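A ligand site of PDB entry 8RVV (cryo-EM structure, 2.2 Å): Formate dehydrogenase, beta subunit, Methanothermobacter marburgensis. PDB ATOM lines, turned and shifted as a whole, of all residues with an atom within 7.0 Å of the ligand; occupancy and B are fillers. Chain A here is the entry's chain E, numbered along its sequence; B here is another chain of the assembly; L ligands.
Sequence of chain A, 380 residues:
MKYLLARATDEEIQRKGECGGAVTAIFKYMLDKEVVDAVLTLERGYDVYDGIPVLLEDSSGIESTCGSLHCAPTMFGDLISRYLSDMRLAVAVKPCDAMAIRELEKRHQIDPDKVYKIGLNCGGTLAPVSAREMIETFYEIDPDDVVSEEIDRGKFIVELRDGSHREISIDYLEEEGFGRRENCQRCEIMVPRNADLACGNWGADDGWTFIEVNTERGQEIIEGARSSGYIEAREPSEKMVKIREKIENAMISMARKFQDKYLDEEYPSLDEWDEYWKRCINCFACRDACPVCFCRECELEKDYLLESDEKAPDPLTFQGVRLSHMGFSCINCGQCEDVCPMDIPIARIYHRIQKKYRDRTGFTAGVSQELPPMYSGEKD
The side-chain sulfur of Cys 340 sits close to the backbone NH of Ile 344, at 3.6 Å.
The backbone NH (N) of Met 342 lies close to the side-chain sulfur (SG) of Cys 340 (3.6 Å).
The backbone NH (N) of Asp 343 lies close to the side-chain sulfur (SG) of Cys 340, at 3.7 Å.
SG of Cys 283 sits close to N of Ala 285, 3.3 Å away.
The guanidinium group (NH1) of Arg 46 of chain B lies within hydrogen-bond range of the backbone carbonyl oxygen (O) of Cys 283.
The backbone NH (N) of Asn 282 sits close to the side-chain sulfur (SG) of Cys 280, at 3.3 Å.
Asn 282 touches the ligand.
Ala 285 touches the ligand.
Phe 318 touches the ligand (CZ to S1, 3.6 Å).
Pro 341 touches the ligand.
Ile 344 touches the ligand (CD1 to S3, 3.9 Å).
Ile 346 touches the ligand.
Hydrophobic or aromatic side chains that line the ligand: Ile 281, Ala 285, Phe 318, Pro 341, Ile 344 and Ile 346.
Within 4 Å of the ligand: Cys 280, Ile 281, Asn 282, Cys 283, Phe 284, Ala 285, Cys 286, Phe 318, Gln 319, Cys 340, Pro 341, Ile 344 and Ile 346.
The side-chain sulfur (SG) of Cys 340 binds an iron atom (FE1) of the ligand.
A sulfur (S1) of the ligand sits close to the backbone NH (N) of Cys 283 (3.3 Å).
The side-chain sulfur (SG) of Cys 283 is bound to an iron atom (FE3) of the ligand (2.3 Å).
An iron atom (FE4) of the ligand is bound by the side-chain sulfur (SG) of Cys 280, at 2.3 Å.
A sulfur (S4) of the ligand sits close to the backbone NH (N) of Cys 286, at 3.3 Å.
The side-chain sulfur (SG) of Cys 286 binds an iron atom (FE2) of the ligand.
The backbone NH (N) of Phe 284 lies close to a sulfur (S1) of the ligand.
A sulfur (S2) of the ligand lies close to the backbone NH (N) of Ile 281, 3.5 Å away.
A sulfur (S3) of the ligand lies close to the side-chain amide nitrogen (NE2) of Gln 319 (3.7 Å).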
ATOM      1  N   TRP A 277      24.521   5.750  -6.110  1.00  0.00           N
ATOM      2  CA  TRP A 277      23.300   4.946  -6.188  1.00  0.00           C
ATOM      3  C   TRP A 277      22.283   5.587  -7.118  1.00  0.00           C
ATOM      4  O   TRP A 277      21.455   4.890  -7.710  1.00  0.00           O
ATOM      5  CB  TRP A 277      22.699   4.744  -4.804  1.00  0.00           C
ATOM      6  CG  TRP A 277      23.579   3.998  -3.822  1.00  0.00           C
ATOM      7  CD1 TRP A 277      23.827   4.342  -2.530  1.00  0.00           C
ATOM      8  CD2 TRP A 277      24.316   2.785  -4.052  1.00  0.00           C
ATOM      9  NE1 TRP A 277      24.667   3.429  -1.945  1.00  0.00           N
ATOM     10  CE2 TRP A 277      24.982   2.469  -2.856  1.00  0.00           C
ATOM     11  CE3 TRP A 277      24.470   1.946  -5.154  1.00  0.00           C
ATOM     12  CZ2 TRP A 277      25.789   1.336  -2.735  1.00  0.00           C
ATOM     13  CZ3 TRP A 277      25.279   0.827  -5.032  1.00  0.00           C
ATOM     14  CH2 TRP A 277      25.930   0.542  -3.828  1.00  0.00           C
ATOM     15  N   ARG A 279      22.781   6.563  -9.944  1.00  0.00           N
ATOM     16  CA  ARG A 279      23.076   6.150 -11.309  1.00  0.00           C
ATOM     17  C   ARG A 279      22.442   4.822 -11.677  1.00  0.00           C
ATOM     18  O   ARG A 279      22.096   4.612 -12.844  1.00  0.00           O
ATOM     19  CB  ARG A 279      24.590   6.035 -11.499  1.00  0.00           C
ATOM     20  CG  ARG A 279      25.313   7.317 -11.752  1.00  0.00           C
ATOM     21  CD  ARG A 279      26.725   7.047 -12.209  1.00  0.00           C
ATOM     22  NE  ARG A 279      27.661   8.046 -11.726  1.00  0.00           N
ATOM     23  CZ  ARG A 279      28.969   7.847 -11.591  1.00  0.00           C
ATOM     24  NH1 ARG A 279      29.521   6.683 -11.893  1.00  0.00           N
ATOM     25  NH2 ARG A 279      29.739   8.839 -11.155  1.00  0.00           N
ATOM     26  N   CYS A 280      22.294   3.920 -10.713  1.00  0.00           N
ATOM     27  CA  CYS A 280      22.028   2.515 -11.009  1.00  0.00           C
ATOM     28  C   CYS A 280      20.864   2.356 -11.982  1.00  0.00           C
ATOM     29  O   CYS A 280      19.805   2.948 -11.802  1.00  0.00           O
ATOM     30  CB  CYS A 280      21.749   1.761  -9.708  1.00  0.00           C
ATOM     31  SG  CYS A 280      21.285   0.033  -9.913  1.00  0.00           S
ATOM     32  N   ILE A 281      21.077   1.545 -13.020  1.00  0.00           N
ATOM     33  CA  ILE A 281      20.067   1.295 -14.037  1.00  0.00           C
ATOM     34  C   ILE A 281      19.367  -0.045 -13.824  1.00  0.00           C
ATOM     35  O   ILE A 281      18.587  -0.467 -14.685  1.00  0.00           O
ATOM     36  CB  ILE A 281      20.666   1.385 -15.449  1.00  0.00           C
ATOM     37  CG1 ILE A 281      21.902   0.481 -15.580  1.00  0.00           C
ATOM     38  CG2 ILE A 281      21.039   2.815 -15.785  1.00  0.00           C
ATOM     39  CD1 ILE A 281      22.079  -0.100 -16.955  1.00  0.00           C
ATOM     40  N   ASN A 282      19.643  -0.724 -12.720  1.00  0.00           N
ATOM     41  CA  ASN A 282      18.911  -1.943 -12.356  1.00  0.00           C
ATOM     42  C   ASN A 282      19.127  -3.056 -13.387  1.00  0.00           C
ATOM     43  O   ASN A 282      18.219  -3.815 -13.701  1.00  0.00           O
ATOM     44  CB  ASN A 282      17.429  -1.637 -12.186  1.00  0.00           C
ATOM     45  CG  ASN A 282      16.748  -2.579 -11.223  1.00  0.00           C
ATOM     46  OD1 ASN A 282      17.251  -2.846 -10.132  1.00  0.00           O
ATOM     47  ND2 ASN A 282      15.579  -3.077 -11.610  1.00  0.00           N
ATOM     48  N   CYS A 283      20.349  -3.140 -13.919  1.00  0.00           N
ATOM     49  CA  CYS A 283      20.655  -4.093 -14.965  1.00  0.00           C
ATOM     50  C   CYS A 283      21.026  -5.474 -14.439  1.00  0.00           C
ATOM     51  O   CYS A 283      21.032  -6.427 -15.211  1.00  0.00           O
ATOM     52  CB  CYS A 283      21.811  -3.562 -15.831  1.00  0.00           C
ATOM     53  SG  CYS A 283      23.414  -3.621 -15.029  1.00  0.00           S
ATOM     54  N   PHE A 284      21.326  -5.591 -13.149  1.00  0.00           N
ATOM     55  CA  PHE A 284      21.690  -6.846 -12.497  1.00  0.00           C
ATOM     56  C   PHE A 284      22.980  -7.444 -13.018  1.00  0.00           C
ATOM     57  O   PHE A 284      23.217  -8.635 -12.870  1.00  0.00           O
ATOM     58  CB  PHE A 284      20.550  -7.880 -12.627  1.00  0.00           C
ATOM     59  CG  PHE A 284      19.342  -7.536 -11.820  1.00  0.00           C
ATOM     60  CD1 PHE A 284      19.270  -7.872 -10.491  1.00  0.00           C
ATOM     61  CD2 PHE A 284      18.288  -6.857 -12.394  1.00  0.00           C
ATOM     62  CE1 PHE A 284      18.161  -7.545  -9.743  1.00  0.00           C
ATOM     63  CE2 PHE A 284      17.176  -6.528 -11.660  1.00  0.00           C
ATOM     64  CZ  PHE A 284      17.111  -6.879 -10.334  1.00  0.00           C
ATOM     65  N   ALA A 285      23.851  -6.619 -13.627  1.00  0.00           N
ATOM     66  CA  ALA A 285      25.143  -7.131 -14.058  1.00  0.00           C
ATOM     67  C   ALA A 285      25.976  -7.573 -12.869  1.00  0.00           C
ATOM     68  O   ALA A 285      26.685  -8.580 -12.938  1.00  0.00           O
ATOM     69  CB  ALA A 285      25.885  -6.068 -14.874  1.00  0.00           C
ATOM     70  N   CYS A 286      25.905  -6.819 -11.766  1.00  0.00           N
ATOM     71  CA  CYS A 286      26.669  -7.170 -10.573  1.00  0.00           C
ATOM     72  C   CYS A 286      26.231  -8.523 -10.024  1.00  0.00           C
ATOM     73  O   CYS A 286      27.058  -9.382  -9.707  1.00  0.00           O
ATOM     74  CB  CYS A 286      26.508  -6.075  -9.518  1.00  0.00           C
ATOM     75  SG  CYS A 286      24.830  -5.449  -9.305  1.00  0.00           S
ATOM     76  N   ARG A 287      24.917  -8.734  -9.902  1.00  0.00           N
ATOM     77  CA  ARG A 287      24.429 -10.004  -9.391  1.00  0.00           C
ATOM     78  C   ARG A 287      24.775 -11.152 -10.331  1.00  0.00           C
ATOM     79  O   ARG A 287      25.167 -12.236  -9.883  1.00  0.00           O
ATOM     80  CB  ARG A 287      22.921  -9.929  -9.156  1.00  0.00           C
ATOM     81  CG  ARG A 287      22.356 -11.160  -8.464  1.00  0.00           C
ATOM     82  CD  ARG A 287      21.065 -11.640  -9.078  1.00  0.00           C
ATOM     83  NE  ARG A 287      21.112 -11.742 -10.534  1.00  0.00           N
ATOM     84  CZ  ARG A 287      20.065 -11.569 -11.325  1.00  0.00           C
ATOM     85  NH1 ARG A 287      18.865 -11.334 -10.830  1.00  0.00           N
ATOM     86  NH2 ARG A 287      20.220 -11.642 -12.640  1.00  0.00           N
ATOM     87  N   PRO A 313      17.022   2.343  -8.641  1.00  0.00           N
ATOM     88  CA  PRO A 313      16.347   1.659  -7.532  1.00  0.00           C
ATOM     89  C   PRO A 313      16.798   2.197  -6.187  1.00  0.00           C
ATOM     90  O   PRO A 313      17.883   2.755  -6.023  1.00  0.00           O
ATOM     91  CB  PRO A 313      16.761   0.197  -7.717  1.00  0.00           C
ATOM     92  CG  PRO A 313      18.060   0.260  -8.407  1.00  0.00           C
ATOM     93  CD  PRO A 313      17.992   1.463  -9.317  1.00  0.00           C
ATOM     94  N   PHE A 318      17.703  -3.323  -2.985  1.00  0.00           N
ATOM     95  CA  PHE A 318      18.539  -4.043  -3.933  1.00  0.00           C
ATOM     96  C   PHE A 318      19.881  -4.418  -3.317  1.00  0.00           C
ATOM     97  O   PHE A 318      20.159  -5.602  -3.083  1.00  0.00           O
ATOM     98  CB  PHE A 318      18.736  -3.145  -5.177  1.00  0.00           C
ATOM     99  CG  PHE A 318      19.462  -3.809  -6.321  1.00  0.00           C
ATOM    100  CD1 PHE A 318      20.821  -4.075  -6.242  1.00  0.00           C
ATOM    101  CD2 PHE A 318      18.800  -4.136  -7.487  1.00  0.00           C
ATOM    102  CE1 PHE A 318      21.492  -4.682  -7.295  1.00  0.00           C
ATOM    103  CE2 PHE A 318      19.465  -4.735  -8.530  1.00  0.00           C
ATOM    104  CZ  PHE A 318      20.804  -5.007  -8.440  1.00  0.00           C
ATOM    105  N   GLN A 319      20.674  -3.411  -2.927  1.00  0.00           N
ATOM    106  CA  GLN A 319      22.001  -3.676  -2.397  1.00  0.00           C
ATOM    107  C   GLN A 319      21.934  -4.257  -0.990  1.00  0.00           C
ATOM    108  O   GLN A 319      22.666  -5.194  -0.683  1.00  0.00           O
ATOM    109  CB  GLN A 319      22.842  -2.397  -2.407  1.00  0.00           C
ATOM    110  CG  GLN A 319      22.907  -1.692  -3.755  1.00  0.00           C
ATOM    111  CD  GLN A 319      23.743  -2.434  -4.779  1.00  0.00           C
ATOM    112  OE1 GLN A 319      24.546  -3.293  -4.427  1.00  0.00           O
ATOM    113  NE2 GLN A 319      23.548  -2.113  -6.045  1.00  0.00           N
ATOM    114  N   ARG A 322      20.799  -7.899  -1.203  1.00  0.00           N
ATOM    115  CA  ARG A 322      21.874  -8.786  -1.641  1.00  0.00           C
ATOM    116  C   ARG A 322      22.940  -8.930  -0.560  1.00  0.00           C
ATOM    117  O   ARG A 322      23.498 -10.024  -0.374  1.00  0.00           O
ATOM    118  CB  ARG A 322      22.484  -8.262  -2.944  1.00  0.00           C
ATOM    119  CG  ARG A 322      23.427  -9.260  -3.622  1.00  0.00           C
ATOM    120  CD  ARG A 322      23.629  -8.953  -5.091  1.00  0.00           C
ATOM    121  NE  ARG A 322      24.843  -8.184  -5.343  1.00  0.00           N
ATOM    122  CZ  ARG A 322      26.067  -8.692  -5.300  1.00  0.00           C
ATOM    123  NH1 ARG A 322      26.282  -9.966  -5.063  1.00  0.00           N
ATOM    124  NH2 ARG A 322      27.102  -7.878  -5.502  1.00  0.00           N
ATOM    125  N   CYS A 336      31.628  -7.894  -9.544  1.00  0.00           N
ATOM    126  CA  CYS A 336      30.477  -7.003  -9.578  1.00  0.00           C
ATOM    127  C   CYS A 336      30.875  -5.608 -10.055  1.00  0.00           C
ATOM    128  O   CYS A 336      30.171  -4.997 -10.865  1.00  0.00           O
ATOM    129  CB  CYS A 336      29.828  -6.924  -8.208  1.00  0.00           C
ATOM    130  SG  CYS A 336      31.002  -6.649  -6.852  1.00  0.00           S
ATOM    131  N   VAL A 339      31.843  -5.262 -14.033  1.00  0.00           N
ATOM    132  CA  VAL A 339      30.822  -5.315 -15.074  1.00  0.00           C
ATOM    133  C   VAL A 339      29.776  -4.225 -14.946  1.00  0.00           C
ATOM    134  O   VAL A 339      28.880  -4.142 -15.794  1.00  0.00           O
ATOM    135  CB  VAL A 339      30.125  -6.692 -15.100  1.00  0.00           C
ATOM    136  CG1 VAL A 339      31.151  -7.806 -15.256  1.00  0.00           C
ATOM    137  CG2 VAL A 339      29.301  -6.907 -13.830  1.00  0.00           C
ATOM    138  N   CYS A 340      29.853  -3.386 -13.922  1.00  0.00           N
ATOM    139  CA  CYS A 340      28.818  -2.393 -13.692  1.00  0.00           C
ATOM    140  C   CYS A 340      28.813  -1.359 -14.818  1.00  0.00           C
ATOM    141  O   CYS A 340      29.817  -0.666 -14.991  1.00  0.00           O
ATOM    142  CB  CYS A 340      29.019  -1.716 -12.349  1.00  0.00           C
ATOM    143  SG  CYS A 340      27.742  -0.523 -11.934  1.00  0.00           S
ATOM    144  N   PRO A 341      27.726  -1.218 -15.581  1.00  0.00           N
ATOM    145  CA  PRO A 341      27.723  -0.206 -16.638  1.00  0.00           C
ATOM    146  C   PRO A 341      27.791   1.219 -16.131  1.00  0.00           C
ATOM    147  O   PRO A 341      28.163   2.119 -16.887  1.00  0.00           O
ATOM    148  CB  PRO A 341      26.391  -0.460 -17.383  1.00  0.00           C
ATOM    149  CG  PRO A 341      25.828  -1.701 -16.816  1.00  0.00           C
ATOM    150  CD  PRO A 341      26.442  -1.927 -15.489  1.00  0.00           C
ATOM    151  N   MET A 342      27.439   1.456 -14.870  1.00  0.00           N
ATOM    152  CA  MET A 342      27.362   2.797 -14.313  1.00  0.00           C
ATOM    153  C   MET A 342      28.585   3.176 -13.486  1.00  0.00           C
ATOM    154  O   MET A 342      28.621   4.278 -12.931  1.00  0.00           O
ATOM    155  CB  MET A 342      26.084   2.919 -13.459  1.00  0.00           C
ATOM    156  CG  MET A 342      24.825   3.372 -14.207  1.00  0.00           C
ATOM    157  SD  MET A 342      25.062   4.533 -15.573  1.00  0.00           S
ATOM    158  CE  MET A 342      24.568   3.548 -16.977  1.00  0.00           C
ATOM    159  N   ASP A 343      29.574   2.298 -13.395  1.00  0.00           N
ATOM    160  CA  ASP A 343      30.829   2.581 -12.688  1.00  0.00           C
ATOM    161  C   ASP A 343      30.588   2.905 -11.215  1.00  0.00           C
ATOM    162  O   ASP A 343      31.010   3.943 -10.699  1.00  0.00           O
ATOM    163  CB  ASP A 343      31.598   3.709 -13.378  1.00  0.00           C
ATOM    164  CG  ASP A 343      32.080   3.340 -14.762  1.00  0.00           C
ATOM    165  OD1 ASP A 343      32.985   2.486 -14.875  1.00  0.00           O
ATOM    166  OD2 ASP A 343      31.573   3.920 -15.734  1.00  0.00           O
ATOM    167  N   ILE A 344      29.912   1.992 -10.519  1.00  0.00           N
ATOM    168  CA  ILE A 344      29.696   2.107  -9.084  1.00  0.00           C
ATOM    169  C   ILE A 344      30.695   1.214  -8.355  1.00  0.00           C
ATOM    170  O   ILE A 344      30.900   0.064  -8.778  1.00  0.00           O
ATOM    171  CB  ILE A 344      28.246   1.758  -8.708  1.00  0.00           C
ATOM    172  CG1 ILE A 344      27.276   2.722  -9.398  1.00  0.00           C
ATOM    173  CG2 ILE A 344      28.059   1.813  -7.206  1.00  0.00           C
ATOM    174  CD1 ILE A 344      25.857   2.225  -9.433  1.00  0.00           C
ATOM    175  N   ILE A 346      30.912  -1.135  -6.035  1.00  0.00           N
ATOM    176  CA  ILE A 346      30.100  -2.030  -5.214  1.00  0.00           C
ATOM    177  C   ILE A 346      30.985  -2.899  -4.321  1.00  0.00           C
ATOM    178  O   ILE A 346      30.678  -3.128  -3.133  1.00  0.00           O
ATOM    179  CB  ILE A 346      29.207  -2.897  -6.127  1.00  0.00           C
ATOM    180  CG1 ILE A 346      28.440  -2.037  -7.134  1.00  0.00           C
ATOM    181  CG2 ILE A 346      28.234  -3.696  -5.303  1.00  0.00           C
ATOM    182  CD1 ILE A 346      28.012  -2.802  -8.380  1.00  0.00           C
ATOM    183  N   THR B  41      27.712  -4.651 -19.793  1.00  0.00           N
ATOM    184  CA  THR B  41      26.517  -4.754 -20.614  1.00  0.00           C
ATOM    185  C   THR B  41      25.294  -4.470 -19.752  1.00  0.00           C
ATOM    186  O   THR B  41      25.290  -4.705 -18.543  1.00  0.00           O
ATOM    187  CB  THR B  41      26.371  -6.140 -21.260  1.00  0.00           C
ATOM    188  OG1 THR B  41      26.662  -7.160 -20.295  1.00  0.00           O
ATOM    189  CG2 THR B  41      27.302  -6.294 -22.437  1.00  0.00           C
ATOM    190  N   CYS B  42      24.253  -3.951 -20.400  1.00  0.00           N
ATOM    191  CA  CYS B  42      22.944  -3.883 -19.786  1.00  0.00           C
ATOM    192  C   CYS B  42      22.289  -5.263 -19.850  1.00  0.00           C
ATOM    193  O   CYS B  42      22.885  -6.235 -20.298  1.00  0.00           O
ATOM    194  CB  CYS B  42      22.099  -2.816 -20.483  1.00  0.00           C
ATOM    195  SG  CYS B  42      21.491  -3.268 -22.111  1.00  0.00           S
ATOM    196  N   ARG B  46      23.204  -9.185 -21.931  1.00  0.00           N
ATOM    197  CA  ARG B  46      23.389 -10.488 -21.312  1.00  0.00           C
ATOM    198  C   ARG B  46      22.283 -11.470 -21.683  1.00  0.00           C
ATOM    199  O   ARG B  46      22.466 -12.679 -21.490  1.00  0.00           O
ATOM    200  CB  ARG B  46      23.459 -10.325 -19.786  1.00  0.00           C
ATOM    201  CG  ARG B  46      24.886 -10.194 -19.280  1.00  0.00           C
ATOM    202  CD  ARG B  46      24.952  -9.616 -17.877  1.00  0.00           C
ATOM    203  NE  ARG B  46      24.643  -8.185 -17.850  1.00  0.00           N
ATOM    204  CZ  ARG B  46      23.604  -7.642 -17.236  1.00  0.00           C
ATOM    205  NH1 ARG B  46      22.700  -8.370 -16.601  1.00  0.00           N
ATOM    206  NH2 ARG B  46      23.465  -6.319 -17.258  1.00  0.00           N
HETATM  207 FE1  LIG L   1      25.657  -1.381 -11.595  1.00  0.00          FE
HETATM  208 FE2  LIG L   1      24.365  -3.522 -10.473  1.00  0.00          FE
HETATM  209 FE3  LIG L   1      23.661  -2.662 -12.971  1.00  0.00          FE
HETATM  210 FE4  LIG L   1      23.051  -1.139 -10.779  1.00  0.00          FE
HETATM  211  S1  LIG L   1      22.249  -3.213 -11.267  1.00  0.00           S
HETATM  212  S2  LIG L   1      23.943  -0.407 -12.736  1.00  0.00           S
HETATM  213  S3  LIG L   1      24.871  -1.542  -9.460  1.00  0.00           S
HETATM  214  S4  LIG L   1      25.666  -3.537 -12.330  1.00  0.00           S
